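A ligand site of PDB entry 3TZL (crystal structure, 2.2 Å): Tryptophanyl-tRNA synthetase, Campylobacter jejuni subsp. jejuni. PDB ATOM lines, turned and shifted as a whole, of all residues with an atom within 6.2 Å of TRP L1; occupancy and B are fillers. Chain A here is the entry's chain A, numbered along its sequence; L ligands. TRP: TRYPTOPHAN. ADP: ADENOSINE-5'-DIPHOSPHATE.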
ATOM      1  N   LEU A   7     -10.459   7.706  -4.074  1.00  0.00           N
ATOM      2  CA  LEU A   7     -10.961   8.065  -5.408  1.00  0.00           C
ATOM      3  C   LEU A   7     -10.304   9.321  -5.977  1.00  0.00           C
ATOM      4  O   LEU A   7     -10.262  10.377  -5.331  1.00  0.00           O
ATOM      5  CB  LEU A   7     -12.474   8.273  -5.382  1.00  0.00           C
ATOM      6  CG  LEU A   7     -13.086   8.784  -6.684  1.00  0.00           C
ATOM      7  CD1 LEU A   7     -13.991   7.718  -7.278  1.00  0.00           C
ATOM      8  CD2 LEU A   7     -13.852  10.074  -6.483  1.00  0.00           C
ATOM      9  N   THR A   8      -9.842   9.217  -7.212  1.00  0.00           N
ATOM     10  CA  THR A   8      -9.161  10.318  -7.871  1.00  0.00           C
ATOM     11  C   THR A   8      -9.792  10.623  -9.227  1.00  0.00           C
ATOM     12  O   THR A   8      -9.841   9.763 -10.099  1.00  0.00           O
ATOM     13  CB  THR A   8      -7.678   9.948  -8.118  1.00  0.00           C
ATOM     14  OG1 THR A   8      -7.189   9.229  -6.987  1.00  0.00           O
ATOM     15  CG2 THR A   8      -6.837  11.201  -8.303  1.00  0.00           C
ATOM     16  N   GLY A   9     -10.250  11.850  -9.419  1.00  0.00           N
ATOM     17  CA  GLY A   9     -10.672  12.290 -10.728  1.00  0.00           C
ATOM     18  C   GLY A   9      -9.462  12.827 -11.473  1.00  0.00           C
ATOM     19  O   GLY A   9      -8.615  13.496 -10.891  1.00  0.00           O
ATOM     20  N   LEU A  10      -9.376  12.543 -12.771  1.00  0.00           N
ATOM     21  CA  LEU A  10      -8.227  12.961 -13.552  1.00  0.00           C
ATOM     22  C   LEU A  10      -8.650  13.875 -14.706  1.00  0.00           C
ATOM     23  O   LEU A  10      -9.454  13.474 -15.569  1.00  0.00           O
ATOM     24  CB  LEU A  10      -7.476  11.741 -14.081  1.00  0.00           C
ATOM     25  CG  LEU A  10      -7.143  10.667 -13.040  1.00  0.00           C
ATOM     26  CD1 LEU A  10      -6.859   9.322 -13.720  1.00  0.00           C
ATOM     27  CD2 LEU A  10      -5.966  11.096 -12.150  1.00  0.00           C
ATOM     28  N   GLN A  11      -8.116  15.092 -14.729  1.00  0.00           N
ATOM     29  CA  GLN A  11      -8.352  16.028 -15.818  1.00  0.00           C
ATOM     30  C   GLN A  11      -7.837  15.473 -17.141  1.00  0.00           C
ATOM     31  O   GLN A  11      -6.718  14.963 -17.211  1.00  0.00           O
ATOM     32  CB  GLN A  11      -7.636  17.351 -15.544  1.00  0.00           C
ATOM     33  CG  GLN A  11      -8.262  18.191 -14.457  1.00  0.00           C
ATOM     34  CD  GLN A  11      -7.488  19.475 -14.214  1.00  0.00           C
ATOM     35  OE1 GLN A  11      -6.315  19.573 -14.581  1.00  0.00           O
ATOM     36  NE2 GLN A  11      -8.146  20.463 -13.607  1.00  0.00           N
ATOM     37  N   PHE A  40     -11.005   8.032 -12.441  1.00  0.00           N
ATOM     38  CA  PHE A  40     -11.812   8.302 -13.616  1.00  0.00           C
ATOM     39  C   PHE A  40     -11.326   9.539 -14.361  1.00  0.00           C
ATOM     40  O   PHE A  40     -10.900  10.513 -13.756  1.00  0.00           O
ATOM     41  CB  PHE A  40     -13.308   8.408 -13.257  1.00  0.00           C
ATOM     42  CG  PHE A  40     -13.650   9.615 -12.421  1.00  0.00           C
ATOM     43  CD1 PHE A  40     -14.095  10.786 -13.013  1.00  0.00           C
ATOM     44  CD2 PHE A  40     -13.536   9.570 -11.033  1.00  0.00           C
ATOM     45  CE1 PHE A  40     -14.413  11.907 -12.254  1.00  0.00           C
ATOM     46  CE2 PHE A  40     -13.844  10.687 -10.260  1.00  0.00           C
ATOM     47  CZ  PHE A  40     -14.295  11.860 -10.875  1.00  0.00           C
ATOM     48  N   ALA A  42     -12.131  12.760 -15.897  1.00  0.00           N
ATOM     49  CA  ALA A  42     -13.255  13.654 -15.633  1.00  0.00           C
ATOM     50  C   ALA A  42     -13.662  14.508 -16.839  1.00  0.00           C
ATOM     51  O   ALA A  42     -13.418  15.694 -16.852  1.00  0.00           O
ATOM     52  CB  ALA A  42     -12.947  14.556 -14.445  1.00  0.00           C
ATOM     53  N   HIS A  45     -16.317  17.431 -16.370  1.00  0.00           N
ATOM     54  CA  HIS A  45     -15.689  18.643 -15.826  1.00  0.00           C
ATOM     55  C   HIS A  45     -14.884  19.413 -16.881  1.00  0.00           C
ATOM     56  O   HIS A  45     -14.831  20.624 -16.851  1.00  0.00           O
ATOM     57  CB  HIS A  45     -14.841  18.287 -14.618  1.00  0.00           C
ATOM     58  CG  HIS A  45     -15.637  18.185 -13.345  1.00  0.00           C
ATOM     59  ND1 HIS A  45     -16.016  16.974 -12.802  1.00  0.00           N
ATOM     60  CD2 HIS A  45     -16.161  19.147 -12.557  1.00  0.00           C
ATOM     61  CE1 HIS A  45     -16.721  17.196 -11.697  1.00  0.00           C
ATOM     62  NE2 HIS A  45     -16.812  18.496 -11.521  1.00  0.00           N
ATOM     63  N   GLN A  82     -15.832   9.369 -16.906  1.00  0.00           N
ATOM     64  CA  GLN A  82     -16.931   9.957 -16.124  1.00  0.00           C
ATOM     65  C   GLN A  82     -18.293   9.802 -16.809  1.00  0.00           C
ATOM     66  O   GLN A  82     -19.254   9.331 -16.185  1.00  0.00           O
ATOM     67  CB  GLN A  82     -16.659  11.450 -15.902  1.00  0.00           C
ATOM     68  CG  GLN A  82     -17.386  12.048 -14.702  1.00  0.00           C
ATOM     69  CD  GLN A  82     -16.987  13.488 -14.445  1.00  0.00           C
ATOM     70  OE1 GLN A  82     -16.431  14.153 -15.311  1.00  0.00           O
ATOM     71  NE2 GLN A  82     -17.293  13.971 -13.248  1.00  0.00           N
ATOM     72  N   LYS A 113     -10.622  31.101 -11.483  1.00  0.00           N
ATOM     73  CA  LYS A 113     -10.754  30.686 -12.886  1.00  0.00           C
ATOM     74  C   LYS A 113     -11.357  31.802 -13.730  1.00  0.00           C
ATOM     75  O   LYS A 113     -11.015  31.962 -14.907  1.00  0.00           O
ATOM     76  CB  LYS A 113     -11.572  29.404 -13.006  1.00  0.00           C
ATOM     77  CG  LYS A 113     -10.749  28.125 -12.833  1.00  0.00           C
ATOM     78  CD  LYS A 113     -11.653  26.914 -12.651  1.00  0.00           C
ATOM     79  CE  LYS A 113     -10.892  25.620 -12.863  1.00  0.00           C
ATOM     80  NZ  LYS A 113     -11.775  24.415 -12.686  1.00  0.00           N
ATOM     81  N   TYR A 127     -19.340  23.555 -10.847  1.00  0.00           N
ATOM     82  CA  TYR A 127     -18.199  22.605 -10.772  1.00  0.00           C
ATOM     83  C   TYR A 127     -18.057  21.821  -9.446  1.00  0.00           C
ATOM     84  O   TYR A 127     -17.964  20.603  -9.462  1.00  0.00           O
ATOM     85  CB  TYR A 127     -16.896  23.352 -11.103  1.00  0.00           C
ATOM     86  CG  TYR A 127     -15.651  22.523 -11.379  1.00  0.00           C
ATOM     87  CD1 TYR A 127     -15.127  22.432 -12.660  1.00  0.00           C
ATOM     88  CD2 TYR A 127     -14.962  21.890 -10.345  1.00  0.00           C
ATOM     89  CE1 TYR A 127     -13.979  21.689 -12.925  1.00  0.00           C
ATOM     90  CE2 TYR A 127     -13.802  21.134 -10.593  1.00  0.00           C
ATOM     91  CZ  TYR A 127     -13.320  21.045 -11.887  1.00  0.00           C
ATOM     92  OH  TYR A 127     -12.173  20.310 -12.163  1.00  0.00           O
ATOM     93  N   LEU A 130     -20.943  19.034  -8.886  1.00  0.00           N
ATOM     94  CA  LEU A 130     -20.749  17.835  -9.684  1.00  0.00           C
ATOM     95  C   LEU A 130     -19.619  16.969  -9.139  1.00  0.00           C
ATOM     96  O   LEU A 130     -19.739  15.739  -9.051  1.00  0.00           O
ATOM     97  CB  LEU A 130     -20.484  18.205 -11.142  1.00  0.00           C
ATOM     98  CG  LEU A 130     -20.266  16.974 -12.024  1.00  0.00           C
ATOM     99  CD1 LEU A 130     -21.493  16.044 -11.985  1.00  0.00           C
ATOM    100  CD2 LEU A 130     -19.918  17.386 -13.440  1.00  0.00           C
ATOM    101  N   MET A 131     -18.517  17.602  -8.749  1.00  0.00           N
ATOM    102  CA  MET A 131     -17.425  16.875  -8.116  1.00  0.00           C
ATOM    103  C   MET A 131     -17.857  16.222  -6.792  1.00  0.00           C
ATOM    104  O   MET A 131     -17.429  15.115  -6.466  1.00  0.00           O
ATOM    105  CB  MET A 131     -16.248  17.807  -7.876  1.00  0.00           C
ATOM    106  CG  MET A 131     -15.015  17.158  -7.187  1.00  0.00           C
ATOM    107  SD  MET A 131     -13.510  18.463  -7.291  1.00  0.00           S
ATOM    108  CE  MET A 131     -14.646  19.994  -7.558  1.00  0.00           C
ATOM    109  N   ASP A 134     -19.423  13.030  -7.758  1.00  0.00           N
ATOM    110  CA  ASP A 134     -18.359  12.062  -8.053  1.00  0.00           C
ATOM    111  C   ASP A 134     -17.902  11.378  -6.768  1.00  0.00           C
ATOM    112  O   ASP A 134     -17.843  10.142  -6.666  1.00  0.00           O
ATOM    113  CB  ASP A 134     -17.140  12.778  -8.658  1.00  0.00           C
ATOM    114  CG  ASP A 134     -17.381  13.328 -10.072  1.00  0.00           C
ATOM    115  OD1 ASP A 134     -18.005  12.630 -10.907  1.00  0.00           O
ATOM    116  OD2 ASP A 134     -16.901  14.441 -10.361  1.00  0.00           O
ATOM    117  N   ILE A 135     -17.539  12.198  -5.785  1.00  0.00           N
ATOM    118  CA  ILE A 135     -16.953  11.706  -4.546  1.00  0.00           C
ATOM    119  C   ILE A 135     -17.952  10.881  -3.734  1.00  0.00           C
ATOM    120  O   ILE A 135     -17.643   9.760  -3.316  1.00  0.00           O
ATOM    121  CB  ILE A 135     -16.421  12.886  -3.701  1.00  0.00           C
ATOM    122  CG1 ILE A 135     -15.326  13.625  -4.473  1.00  0.00           C
ATOM    123  CG2 ILE A 135     -15.902  12.397  -2.336  1.00  0.00           C
ATOM    124  CD1 ILE A 135     -14.983  15.008  -3.901  1.00  0.00           C
ATOM    125  N   VAL A 143      -9.616  11.561  -0.893  1.00  0.00           N
ATOM    126  CA  VAL A 143      -9.510  12.142  -2.224  1.00  0.00           C
ATOM    127  C   VAL A 143      -8.115  12.767  -2.480  1.00  0.00           C
ATOM    128  O   VAL A 143      -7.829  13.884  -2.062  1.00  0.00           O
ATOM    129  CB  VAL A 143     -10.600  13.226  -2.467  1.00  0.00           C
ATOM    130  CG1 VAL A 143     -10.681  13.625  -3.940  1.00  0.00           C
ATOM    131  CG2 VAL A 143     -11.977  12.752  -1.971  1.00  0.00           C
ATOM    132  N   PRO A 144      -7.231  12.022  -3.162  1.00  0.00           N
ATOM    133  CA  PRO A 144      -5.910  12.601  -3.446  1.00  0.00           C
ATOM    134  C   PRO A 144      -6.015  13.825  -4.361  1.00  0.00           C
ATOM    135  O   PRO A 144      -6.516  13.699  -5.479  1.00  0.00           O
ATOM    136  CB  PRO A 144      -5.184  11.471  -4.162  1.00  0.00           C
ATOM    137  CG  PRO A 144      -5.843  10.240  -3.671  1.00  0.00           C
ATOM    138  CD  PRO A 144      -7.294  10.597  -3.528  1.00  0.00           C
ATOM    139  N   VAL A 145      -5.578  14.979  -3.890  1.00  0.00           N
ATOM    140  CA  VAL A 145      -5.675  16.214  -4.677  1.00  0.00           C
ATOM    141  C   VAL A 145      -4.490  17.151  -4.476  1.00  0.00           C
ATOM    142  O   VAL A 145      -3.730  17.033  -3.513  1.00  0.00           O
ATOM    143  CB  VAL A 145      -6.957  17.012  -4.334  1.00  0.00           C
ATOM    144  CG1 VAL A 145      -8.176  16.384  -4.982  1.00  0.00           C
ATOM    145  CG2 VAL A 145      -7.132  17.140  -2.813  1.00  0.00           C
ATOM    146  N   GLN A 149      -7.417  22.086  -4.752  1.00  0.00           N
ATOM    147  CA  GLN A 149      -8.670  21.344  -4.849  1.00  0.00           C
ATOM    148  C   GLN A 149      -9.169  20.911  -3.466  1.00  0.00           C
ATOM    149  O   GLN A 149     -10.195  20.241  -3.344  1.00  0.00           O
ATOM    150  CB  GLN A 149      -8.532  20.139  -5.769  1.00  0.00           C
ATOM    151  CG  GLN A 149      -8.300  20.492  -7.245  1.00  0.00           C
ATOM    152  CD  GLN A 149      -9.503  21.137  -7.913  1.00  0.00           C
ATOM    153  OE1 GLN A 149     -10.637  20.650  -7.772  1.00  0.00           O
ATOM    154  NE2 GLN A 149      -9.288  22.233  -8.630  1.00  0.00           N
ATOM    155  N   HIS A 152     -12.721  22.204  -2.512  1.00  0.00           N
ATOM    156  CA  HIS A 152     -13.734  21.414  -3.203  1.00  0.00           C
ATOM    157  C   HIS A 152     -14.082  20.134  -2.442  1.00  0.00           C
ATOM    158  O   HIS A 152     -15.240  19.742  -2.373  1.00  0.00           O
ATOM    159  CB  HIS A 152     -13.237  21.036  -4.585  1.00  0.00           C
ATOM    160  CG  HIS A 152     -13.293  22.163  -5.568  1.00  0.00           C
ATOM    161  ND1 HIS A 152     -12.510  22.192  -6.710  1.00  0.00           N
ATOM    162  CD2 HIS A 152     -14.055  23.277  -5.608  1.00  0.00           C
ATOM    163  CE1 HIS A 152     -12.783  23.285  -7.397  1.00  0.00           C
ATOM    164  NE2 HIS A 152     -13.719  23.959  -6.744  1.00  0.00           N
ATOM    165  N   VAL A 153     -13.074  19.473  -1.906  1.00  0.00           N
ATOM    166  CA  VAL A 153     -13.316  18.257  -1.141  1.00  0.00           C
ATOM    167  C   VAL A 153     -14.068  18.642   0.129  1.00  0.00           C
ATOM    168  O   VAL A 153     -15.017  17.961   0.540  1.00  0.00           O
ATOM    169  CB  VAL A 153     -11.998  17.560  -0.790  1.00  0.00           C
ATOM    170  CG1 VAL A 153     -12.260  16.351   0.084  1.00  0.00           C
ATOM    171  CG2 VAL A 153     -11.302  17.160  -2.076  1.00  0.00           C
HETATM  172  N   TRP L   1     -11.325  18.842 -10.001  1.00  0.00           N
HETATM  173  CA  TRP L   1     -10.307  17.832 -10.263  1.00  0.00           C
HETATM  174  C   TRP L   1      -9.078  18.452 -10.917  1.00  0.00           C
HETATM  175  O   TRP L   1      -8.071  17.760 -11.115  1.00  0.00           O
HETATM  176  CB  TRP L   1     -10.858  16.721 -11.154  1.00  0.00           C
HETATM  177  CG  TRP L   1     -11.986  16.005 -10.510  1.00  0.00           C
HETATM  178  CD1 TRP L   1     -13.272  15.924 -10.959  1.00  0.00           C
HETATM  179  CD2 TRP L   1     -11.937  15.246  -9.299  1.00  0.00           C
HETATM  180  NE1 TRP L   1     -14.017  15.161 -10.108  1.00  0.00           N
HETATM  181  CE2 TRP L   1     -13.222  14.722  -9.074  1.00  0.00           C
HETATM  182  CE3 TRP L   1     -10.909  14.933  -8.388  1.00  0.00           C
HETATM  183  CZ2 TRP L   1     -13.527  13.935  -7.969  1.00  0.00           C
HETATM  184  CZ3 TRP L   1     -11.211  14.144  -7.292  1.00  0.00           C
HETATM  185  CH2 TRP L   1     -12.513  13.650  -7.097  1.00  0.00           C
HETATM  186  OXT TRP L   1      -9.097  19.635 -11.263  1.00  0.00           O
HETATM  187  PB  ADP L   2      -0.231  21.433 -14.015  1.00  0.00           P
HETATM  188  O1B ADP L   2       1.056  21.558 -13.381  1.00  0.00           O
HETATM  189  O2B ADP L   2       0.079  21.631 -15.396  1.00  0.00           O
HETATM  190  O3B ADP L   2      -0.891  22.678 -13.713  1.00  0.00           O
HETATM  191  PA  ADP L   2      -1.965  19.898 -12.660  1.00  0.00           P
HETATM  192  O1A ADP L   2      -3.291  19.743 -13.218  1.00  0.00           O
HETATM  193  O2A ADP L   2      -2.138  21.111 -11.836  1.00  0.00           O
HETATM  194  O3A ADP L   2      -0.955  20.124 -13.798  1.00  0.00           O
HETATM  195  O5' ADP L   2      -1.658  18.667 -11.777  1.00  0.00           O
HETATM  196  C5' ADP L   2      -1.644  18.825 -10.433  1.00  0.00           C
HETATM  197  C4' ADP L   2      -1.129  17.564  -9.830  1.00  0.00           C
HETATM  198  O4' ADP L   2       0.065  17.095 -10.355  1.00  0.00           O
HETATM  199  C3' ADP L   2      -0.919  17.716  -8.362  1.00  0.00           C
HETATM  200  O3' ADP L   2      -1.005  16.505  -7.782  1.00  0.00           O
HETATM  201  C2' ADP L   2       0.464  18.105  -8.299  1.00  0.00           C
HETATM  202  O2' ADP L   2       1.009  17.630  -7.149  1.00  0.00           O
HETATM  203  C1' ADP L   2       1.051  17.419  -9.459  1.00  0.00           C
HETATM  204  N9  ADP L   2       1.991  18.297 -10.042  1.00  0.00           N
HETATM  205  C8  ADP L   2       1.780  19.107 -11.099  1.00  0.00           C
HETATM  206  N7  ADP L   2       2.857  19.803 -11.376  1.00  0.00           N
HETATM  207  C5  ADP L   2       3.834  19.473 -10.500  1.00  0.00           C
HETATM  208  C6  ADP L   2       5.153  19.880 -10.300  1.00  0.00           C
HETATM  209  N6  ADP L   2       5.766  20.819 -11.118  1.00  0.00           N
HETATM  210  N1  ADP L   2       5.801  19.333  -9.299  1.00  0.00           N
HETATM  211  C2  ADP L   2       5.263  18.439  -8.505  1.00  0.00           C
HETATM  212  N3  ADP L   2       4.033  18.033  -8.656  1.00  0.00           N
HETATM  213  C4  ADP L   2       3.292  18.519  -9.627  1.00  0.00           C
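An oxygen (OXT) of TRP L1 is in hydrogen-bond range of the side-chain amide nitrogen of Gln 11 (2.7 Å).
The side-chain sulfur (SD) of Met 131 is in hydrogen-bond range of a nitrogen (N) of TRP L1.
N of TRP L1 sits at hydrogen-bond distance from OE1 of Gln 149 (3.0 Å).
OH of Tyr 127 is in hydrogen-bond range of N of TRP L1, 2.7 Å away.
The side-chain amide oxygen (OE1) of Gln 11 sits close to an oxygen (O1A) of ADP L2, 3.3 Å away.
A nitrogen (NE1) of TRP L1 is in hydrogen-bond range of the side-chain carboxylate of Asp 134 (3.0 Å).
The side-chain amide oxygen of Gln 149 is in hydrogen-bond range of a ring nitrogen (ND1) of His 152, at 2.6 Å.
The backbone NH (N) of Ala 42 is in hydrogen-bond range of the backbone carbonyl oxygen (O) of Leu 10 (2.8 Å).
The side-chain sulfur of Met 131 lies close to the side-chain amide oxygen of Gln 149.
O of Phe 40 is in hydrogen-bond range of N of Leu 10, at 2.7 Å.
O of Thr 8 lies within hydrogen-bond range of N of Phe 40, 3.1 Å away.
A ring nitrogen (NE2) of His 45 lies within hydrogen-bond range of the backbone NH (N) of Met 131 (3.4 Å).
NE2 of Gln 82 is in hydrogen-bond range of ND1 of His 45 (3.3 Å).
OD1 of Asp 134 sits at hydrogen-bond distance from NE2 of Gln 82 (2.8 Å).
Leu 7 touches TRP L1.
Gly 9 touches TRP L1.
Phe 40 touches TRP L1 (CZ to NE1, 3.4 Å).
Ala 42 touches TRP L1.
His 45 touches TRP L1 (ND1 to CD1, 3.5 Å).
CG1 of Ile 135 touches CH2 of TRP L1, at 3.8 Å.
Val 143 touches TRP L1.
Hydrophobic or aromatic side chains that line TRP L1: Leu 7, Phe 40, Ala 42, His 45, Tyr 127, Met 131, Ile 135 and Val 143.
Of the 21 residues printed, 12 come within 4 Å of TRP L1.
The nearest printed residue that does not touch TRP L1 is Thr 8 (4.3 Å).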
